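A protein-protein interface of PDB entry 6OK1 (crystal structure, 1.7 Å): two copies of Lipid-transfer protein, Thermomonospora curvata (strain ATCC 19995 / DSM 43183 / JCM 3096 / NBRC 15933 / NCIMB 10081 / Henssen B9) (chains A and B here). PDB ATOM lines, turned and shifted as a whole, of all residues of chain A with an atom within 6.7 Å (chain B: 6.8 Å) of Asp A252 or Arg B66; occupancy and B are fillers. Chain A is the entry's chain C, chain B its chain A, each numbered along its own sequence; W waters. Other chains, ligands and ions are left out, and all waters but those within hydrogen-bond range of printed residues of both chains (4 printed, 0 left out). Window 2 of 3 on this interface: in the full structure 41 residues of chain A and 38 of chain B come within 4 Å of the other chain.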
ATOM      1  N   GLY A 250      21.674  -1.748 -22.929  1.00  0.00           N
ATOM      2  CA  GLY A 250      20.318  -2.110 -22.597  1.00  0.00           C
ATOM      3  C   GLY A 250      20.214  -2.794 -21.248  1.00  0.00           C
ATOM      4  O   GLY A 250      21.203  -3.099 -20.586  1.00  0.00           O
ATOM      5  N   TYR A 251      18.967  -3.062 -20.870  1.00  0.00           N
ATOM      6  CA  TYR A 251      18.713  -3.886 -19.701  1.00  0.00           C
ATOM      7  C   TYR A 251      19.351  -5.254 -19.877  1.00  0.00           C
ATOM      8  O   TYR A 251      19.292  -5.851 -20.953  1.00  0.00           O
ATOM      9  CB  TYR A 251      17.207  -4.041 -19.479  1.00  0.00           C
ATOM     10  CG  TYR A 251      16.849  -4.997 -18.366  1.00  0.00           C
ATOM     11  CD1 TYR A 251      16.493  -6.312 -18.639  1.00  0.00           C
ATOM     12  CD2 TYR A 251      16.860  -4.582 -17.039  1.00  0.00           C
ATOM     13  CE1 TYR A 251      16.159  -7.190 -17.622  1.00  0.00           C
ATOM     14  CE2 TYR A 251      16.522  -5.453 -16.016  1.00  0.00           C
ATOM     15  CZ  TYR A 251      16.179  -6.753 -16.311  1.00  0.00           C
ATOM     16  OH  TYR A 251      15.851  -7.613 -15.285  1.00  0.00           O
ATOM     17  N   ASP A 252      19.965  -5.739 -18.800  1.00  0.00           N
ATOM     18  CA  ASP A 252      20.665  -7.023 -18.753  1.00  0.00           C
ATOM     19  C   ASP A 252      21.603  -7.180 -19.944  1.00  0.00           C
ATOM     20  O   ASP A 252      21.553  -8.160 -20.683  1.00  0.00           O
ATOM     21  CB  ASP A 252      19.691  -8.204 -18.691  1.00  0.00           C
ATOM     22  CG  ASP A 252      20.387  -9.496 -18.299  1.00  0.00           C
ATOM     23  OD1 ASP A 252      21.369  -9.429 -17.536  1.00  0.00           O
ATOM     24  OD2 ASP A 252      19.954 -10.581 -18.735  1.00  0.00           O
ATOM     25  N   GLN A 253      22.471  -6.197 -20.116  1.00  0.00           N
ATOM     26  CA  GLN A 253      23.413  -6.196 -21.221  1.00  0.00           C
ATOM     27  C   GLN A 253      24.615  -7.075 -20.910  1.00  0.00           C
ATOM     28  O   GLN A 253      25.221  -6.969 -19.838  1.00  0.00           O
ATOM     29  CB  GLN A 253      23.880  -4.767 -21.507  1.00  0.00           C
ATOM     30  CG  GLN A 253      24.816  -4.631 -22.721  1.00  0.00           C
ATOM     31  CD  GLN A 253      24.056  -4.713 -24.039  1.00  0.00           C
ATOM     32  OE1 GLN A 253      23.047  -4.035 -24.237  1.00  0.00           O
ATOM     33  NE2 GLN A 253      24.549  -5.536 -24.949  1.00  0.00           N
ATOM     34  N   HIS A 254      24.992  -7.904 -21.880  1.00  0.00           N
ATOM     35  CA  HIS A 254      26.223  -8.662 -21.850  1.00  0.00           C
ATOM     36  C   HIS A 254      27.093  -8.312 -23.050  1.00  0.00           C
ATOM     37  O   HIS A 254      26.684  -7.610 -23.974  1.00  0.00           O
ATOM     38  CB  HIS A 254      25.925 -10.161 -21.818  1.00  0.00           C
ATOM     39  CG  HIS A 254      25.146 -10.570 -20.605  1.00  0.00           C
ATOM     40  ND1 HIS A 254      25.728 -11.215 -19.533  1.00  0.00           N
ATOM     41  CD2 HIS A 254      23.857 -10.346 -20.263  1.00  0.00           C
ATOM     42  CE1 HIS A 254      24.807 -11.413 -18.602  1.00  0.00           C
ATOM     43  NE2 HIS A 254      23.668 -10.886 -19.014  1.00  0.00           N
ATOM     44  N   THR A 257      26.607 -11.487 -25.767  1.00  0.00           N
ATOM     45  CA  THR A 257      25.857 -12.678 -25.368  1.00  0.00           C
ATOM     46  C   THR A 257      24.675 -12.356 -24.447  1.00  0.00           C
ATOM     47  O   THR A 257      24.446 -13.047 -23.453  1.00  0.00           O
ATOM     48  CB  THR A 257      26.803 -13.672 -24.692  1.00  0.00           C
ATOM     49  OG1 THR A 257      27.426 -13.092 -23.538  1.00  0.00           O
ATOM     50  CG2 THR A 257      27.906 -14.120 -25.665  1.00  0.00           C
ATOM     51  N   SER A 258      23.899 -11.320 -24.790  1.00  0.00           N
ATOM     52  CA  SER A 258      22.695 -10.916 -24.051  1.00  0.00           C
ATOM     53  C   SER A 258      21.544 -11.854 -24.396  1.00  0.00           C
ATOM     54  O   SER A 258      20.551 -11.479 -25.026  1.00  0.00           O
ATOM     55  CB  SER A 258      22.317  -9.472 -24.365  1.00  0.00           C
ATOM     56  OG  SER A 258      23.401  -8.595 -24.096  1.00  0.00           O
ATOM     57  N   TYR A 259      21.685 -13.085 -23.916  1.00  0.00           N
ATOM     58  CA  TYR A 259      20.772 -14.178 -24.222  1.00  0.00           C
ATOM     59  C   TYR A 259      19.657 -14.365 -23.191  1.00  0.00           C
ATOM     60  O   TYR A 259      18.890 -15.328 -23.305  1.00  0.00           O
ATOM     61  CB  TYR A 259      21.566 -15.478 -24.308  1.00  0.00           C
ATOM     62  CG  TYR A 259      22.652 -15.538 -25.364  1.00  0.00           C
ATOM     63  CD1 TYR A 259      22.545 -14.809 -26.555  1.00  0.00           C
ATOM     64  CD2 TYR A 259      23.778 -16.325 -25.177  1.00  0.00           C
ATOM     65  CE1 TYR A 259      23.528 -14.889 -27.517  1.00  0.00           C
ATOM     66  CE2 TYR A 259      24.769 -16.400 -26.131  1.00  0.00           C
ATOM     67  CZ  TYR A 259      24.643 -15.668 -27.290  1.00  0.00           C
ATOM     68  OH  TYR A 259      25.635 -15.777 -28.230  1.00  0.00           O
ATOM     69  N   TYR A 260      19.549 -13.493 -22.190  1.00  0.00           N
ATOM     70  CA  TYR A 260      18.725 -13.758 -21.009  1.00  0.00           C
ATOM     71  C   TYR A 260      17.569 -12.785 -20.886  1.00  0.00           C
ATOM     72  O   TYR A 260      16.772 -12.879 -19.936  1.00  0.00           O
ATOM     73  CB  TYR A 260      19.627 -13.729 -19.769  1.00  0.00           C
ATOM     74  CG  TYR A 260      20.906 -14.505 -20.003  1.00  0.00           C
ATOM     75  CD1 TYR A 260      20.939 -15.898 -19.869  1.00  0.00           C
ATOM     76  CD2 TYR A 260      22.081 -13.866 -20.408  1.00  0.00           C
ATOM     77  CE1 TYR A 260      22.116 -16.627 -20.095  1.00  0.00           C
ATOM     78  CE2 TYR A 260      23.260 -14.589 -20.637  1.00  0.00           C
ATOM     79  CZ  TYR A 260      23.262 -15.973 -20.492  1.00  0.00           C
ATOM     80  OH  TYR A 260      24.390 -16.726 -20.717  1.00  0.00           O
ATOM     81  N   ARG A 261      17.432 -11.883 -21.850  1.00  0.00           N
ATOM     82  CA  ARG A 261      16.316 -10.959 -21.931  1.00  0.00           C
ATOM     83  C   ARG A 261      15.039 -11.671 -22.351  1.00  0.00           C
ATOM     84  O   ARG A 261      15.069 -12.754 -22.934  1.00  0.00           O
ATOM     85  CB  ARG A 261      16.612  -9.853 -22.950  1.00  0.00           C
ATOM     86  CG  ARG A 261      17.783  -9.024 -22.563  1.00  0.00           C
ATOM     87  CD  ARG A 261      18.510  -8.403 -23.755  1.00  0.00           C
ATOM     88  NE  ARG A 261      19.360  -7.317 -23.283  1.00  0.00           N
ATOM     89  CZ  ARG A 261      20.093  -6.523 -24.059  1.00  0.00           C
ATOM     90  NH1 ARG A 261      20.175  -6.718 -25.371  1.00  0.00           N
ATOM     91  NH2 ARG A 261      20.785  -5.546 -23.506  1.00  0.00           N
ATOM     92  N   GLU B  61      31.067  -1.466 -16.813  1.00  0.00           N
ATOM     93  CA  GLU B  61      29.817  -0.755 -16.619  1.00  0.00           C
ATOM     94  C   GLU B  61      28.632  -1.704 -16.719  1.00  0.00           C
ATOM     95  O   GLU B  61      27.683  -1.599 -15.942  1.00  0.00           O
ATOM     96  CB  GLU B  61      29.683   0.369 -17.662  1.00  0.00           C
ATOM     97  CG  GLU B  61      30.863   1.359 -17.651  1.00  0.00           C
ATOM     98  CD  GLU B  61      31.936   1.036 -18.648  1.00  0.00           C
ATOM     99  OE1 GLU B  61      32.236  -0.165 -18.853  1.00  0.00           O
ATOM    100  OE2 GLU B  61      32.483   1.992 -19.239  1.00  0.00           O
ATOM    101  N   ILE B  62      28.682  -2.654 -17.658  1.00  0.00           N
ATOM    102  CA  ILE B  62      27.519  -3.527 -17.826  1.00  0.00           C
ATOM    103  C   ILE B  62      27.387  -4.501 -16.664  1.00  0.00           C
ATOM    104  O   ILE B  62      26.270  -4.881 -16.294  1.00  0.00           O
ATOM    105  CB  ILE B  62      27.567  -4.284 -19.158  1.00  0.00           C
ATOM    106  CG1 ILE B  62      28.849  -5.111 -19.298  1.00  0.00           C
ATOM    107  CG2 ILE B  62      27.384  -3.289 -20.317  1.00  0.00           C
ATOM    108  CD1 ILE B  62      28.814  -6.054 -20.520  1.00  0.00           C
ATOM    109  N   HIS B  63      28.502  -4.937 -16.087  1.00  0.00           N
ATOM    110  CA  HIS B  63      28.420  -5.858 -14.958  1.00  0.00           C
ATOM    111  C   HIS B  63      27.936  -5.142 -13.712  1.00  0.00           C
ATOM    112  O   HIS B  63      27.089  -5.663 -12.975  1.00  0.00           O
ATOM    113  CB  HIS B  63      29.778  -6.513 -14.727  1.00  0.00           C
ATOM    114  CG  HIS B  63      30.148  -7.465 -15.817  1.00  0.00           C
ATOM    115  ND1 HIS B  63      29.310  -8.494 -16.199  1.00  0.00           N
ATOM    116  CD2 HIS B  63      31.214  -7.519 -16.646  1.00  0.00           C
ATOM    117  CE1 HIS B  63      29.863  -9.155 -17.203  1.00  0.00           C
ATOM    118  NE2 HIS B  63      31.024  -8.589 -17.488  1.00  0.00           N
ATOM    119  N   VAL B  64      28.412  -3.920 -13.486  1.00  0.00           N
ATOM    120  CA  VAL B  64      27.866  -3.112 -12.397  1.00  0.00           C
ATOM    121  C   VAL B  64      26.374  -2.871 -12.615  1.00  0.00           C
ATOM    122  O   VAL B  64      25.558  -2.981 -11.683  1.00  0.00           O
ATOM    123  CB  VAL B  64      28.659  -1.790 -12.269  1.00  0.00           C
ATOM    124  CG1 VAL B  64      28.008  -0.841 -11.266  1.00  0.00           C
ATOM    125  CG2 VAL B  64      30.092  -2.103 -11.835  1.00  0.00           C
ATOM    126  N   ALA B  65      25.986  -2.536 -13.841  1.00  0.00           N
ATOM    127  CA  ALA B  65      24.603  -2.142 -14.061  1.00  0.00           C
ATOM    128  C   ALA B  65      23.649  -3.320 -13.869  1.00  0.00           C
ATOM    129  O   ALA B  65      22.579  -3.150 -13.287  1.00  0.00           O
ATOM    130  CB  ALA B  65      24.437  -1.534 -15.444  1.00  0.00           C
ATOM    131  N   ARG B  66      23.988  -4.511 -14.373  1.00  0.00           N
ATOM    132  CA  ARG B  66      23.036  -5.614 -14.252  1.00  0.00           C
ATOM    133  C   ARG B  66      23.002  -6.178 -12.841  1.00  0.00           C
ATOM    134  O   ARG B  66      21.987  -6.765 -12.438  1.00  0.00           O
ATOM    135  CB  ARG B  66      23.334  -6.719 -15.266  1.00  0.00           C
ATOM    136  CG  ARG B  66      24.566  -7.565 -15.014  1.00  0.00           C
ATOM    137  CD  ARG B  66      24.688  -8.702 -16.059  1.00  0.00           C
ATOM    138  NE  ARG B  66      23.613  -9.687 -15.899  1.00  0.00           N
ATOM    139  CZ  ARG B  66      23.698 -10.770 -15.116  1.00  0.00           C
ATOM    140  NH1 ARG B  66      24.818 -11.029 -14.450  1.00  0.00           N
ATOM    141  NH2 ARG B  66      22.675 -11.618 -15.022  1.00  0.00           N
ATOM    142  N   ASN B  67      24.055  -5.969 -12.058  1.00  0.00           N
ATOM    143  CA  ASN B  67      24.039  -6.422 -10.669  1.00  0.00           C
ATOM    144  C   ASN B  67      23.250  -5.474  -9.782  1.00  0.00           C
ATOM    145  O   ASN B  67      22.558  -5.921  -8.865  1.00  0.00           O
ATOM    146  CB  ASN B  67      25.475  -6.557 -10.145  1.00  0.00           C
ATOM    147  CG  ASN B  67      26.058  -7.935 -10.399  1.00  0.00           C
ATOM    148  OD1 ASN B  67      25.920  -8.820  -9.571  1.00  0.00           O
ATOM    149  ND2 ASN B  67      26.704  -8.122 -11.544  1.00  0.00           N
ATOM    150  N   THR B  68      23.372  -4.167 -10.010  1.00  0.00           N
ATOM    151  CA  THR B  68      22.793  -3.173  -9.112  1.00  0.00           C
ATOM    152  C   THR B  68      21.385  -2.743  -9.484  1.00  0.00           C
ATOM    153  O   THR B  68      20.747  -2.055  -8.679  1.00  0.00           O
ATOM    154  CB  THR B  68      23.655  -1.920  -9.056  1.00  0.00           C
ATOM    155  OG1 THR B  68      23.767  -1.356 -10.378  1.00  0.00           O
ATOM    156  CG2 THR B  68      25.023  -2.254  -8.489  1.00  0.00           C
ATOM    157  N   GLY B  69      20.893  -3.098 -10.669  1.00  0.00           N
ATOM    158  CA  GLY B  69      19.599  -2.615 -11.112  1.00  0.00           C
ATOM    159  C   GLY B  69      19.620  -1.246 -11.748  1.00  0.00           C
ATOM    160  O   GLY B  69      18.546  -0.654 -11.948  1.00  0.00           O
ATOM    161  N   ILE B  70      20.809  -0.729 -12.081  1.00  0.00           N
ATOM    162  CA  ILE B  70      20.919   0.509 -12.853  1.00  0.00           C
ATOM    163  C   ILE B  70      20.293   0.342 -14.230  1.00  0.00           C
ATOM    164  O   ILE B  70      19.758   1.302 -14.808  1.00  0.00           O
ATOM    165  CB  ILE B  70      22.413   0.921 -12.911  1.00  0.00           C
ATOM    166  CG1 ILE B  70      22.804   1.523 -11.570  1.00  0.00           C
ATOM    167  CG2 ILE B  70      22.699   1.874 -14.060  1.00  0.00           C
ATOM    168  CD1 ILE B  70      24.307   1.713 -11.373  1.00  0.00           C
ATOM    169  N   GLY B  71      20.360  -0.860 -14.787  1.00  0.00           N
ATOM    170  CA  GLY B  71      19.658  -1.123 -16.038  1.00  0.00           C
ATOM    171  C   GLY B  71      20.321  -0.432 -17.221  1.00  0.00           C
ATOM    172  O   GLY B  71      21.537  -0.498 -17.407  1.00  0.00           O
ATOM    173  N   GLU B  72      19.522   0.273 -18.016  1.00  0.00           N
ATOM    174  CA  GLU B  72      20.016   0.885 -19.239  1.00  0.00           C
ATOM    175  C   GLU B  72      20.983   2.013 -18.930  1.00  0.00           C
ATOM    176  O   GLU B  72      20.883   2.676 -17.897  1.00  0.00           O
ATOM    177  CB  GLU B  72      18.861   1.459 -20.065  1.00  0.00           C
ATOM    178  CG  GLU B  72      17.904   0.447 -20.636  1.00  0.00           C
ATOM    179  CD  GLU B  72      16.709   1.134 -21.285  1.00  0.00           C
ATOM    180  OE1 GLU B  72      16.155   2.069 -20.671  1.00  0.00           O
ATOM    181  OE2 GLU B  72      16.356   0.784 -22.425  1.00  0.00           O
HETATM  182  O   HOH W   1      23.256  -1.772 -19.384  1.00  0.00           O
HETATM  183  O   HOH W   2      16.967  -2.456 -22.697  1.00  0.00           O
HETATM  184  O   HOH W   3      23.925  -4.557 -18.016  1.00  0.00           O
HETATM  185  O   HOH W   4      20.514 -12.332 -16.710  1.00  0.00           O
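NE of Arg B66 is in salt-bridge range of OD1 of Asp A252.
The guanidinium group (NE) of Arg B66 sits at hydrogen-bond distance from a ring nitrogen (NE2) of His A254, 3.3 Å away.
The backbone NH (N) of Gly A250 lies within hydrogen-bond range of the side-chain amide oxygen (OE1) of Gln A253 (3.0 Å).
O of Tyr A251 is in hydrogen-bond range of NE of Arg A261, at 2.8 Å.
NE2 of His A254 lies within hydrogen-bond range of OD1 of Asp A252, at 3.1 Å.
The side-chain amide nitrogen (NE2) of Gln A253 sits at hydrogen-bond distance from the side-chain hydroxyl (OG) of Ser A258 (3.4 Å).
The side-chain amide oxygen (OE1) of Gln A253 lies within hydrogen-bond range of the guanidinium group (NH2) of Arg A261 (2.8 Å).
The backbone NH (N) of His A254 is in hydrogen-bond range of the side-chain hydroxyl (OG) of Ser A258, at 2.8 Å.
Among the printed residues, merely in contact across the chains: Gln A253 with Ile B62 (3.6 Å), Tyr A251 with Glu B72 (3.7 Å) and His A254 with Ile B62 (3.8 Å).
Of chain B, only Arg B66 comes within 4 Å of Asp A252.
Of chain A, only Asp A252 and His A254 come within 4 Å of Arg B66.
Of the printed residues of chain B, Tyr A251 touches Glu B72.
Printed residues of chain B within 4 Å of His A254: Ile B62 (3.8 Å) and Arg B66 (3.3 Å).
Printed residues of chain A within 4 Å of Glu B72: Tyr A251.
Of the printed residues of chain B, Gln A253 touches Ile B62.
Of the printed residues of chain A, Ile B62 touches Gln A253 (3.6 Å) and His A254 (3.8 Å).
Gly B71 touches none of the printed residues of chain A.
His B63 touches none of the printed residues of chain A.
The nearest printed residue of chain A that does not touch Glu B72 is Gly A250 (4.03 Å).
Of the 10 printed residues of chain A, 4 touch a printed residue of chain B.
Printed residues of chain A that touch a printed residue of chain B: Tyr A251, Asp A252, Gln A253 and His A254.
Hydrophobic or aromatic side chains of chain B within 4 Å of the printed part of chain A: Ile B62.
Among the printed residues, 5 pairs touch across the chains.
No position is printed for both chains.
Of the 5 pairs that touch across the chains among the printed residues, none has its exchanged pair printed and touching as well.
Water W1 lies within hydrogen-bond range of O of Gly A250 and O of Gly B71.
Water W4 lies within hydrogen-bond range of OD2 of Asp A252 (2.7 Å) and NH2 of Arg B66 (2.8 Å).
Water W2 lies within hydrogen-bond range of the backbone NH (N) of Tyr A251 (2.8 Å) and the side-chain carboxylate (OE2) of Glu B72 (3.3 Å).
Water W3 bridges the backbone carbonyl oxygen of Ile B62 (2.9 Å) and the backbone NH of Gln A253 (3.0 Å).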
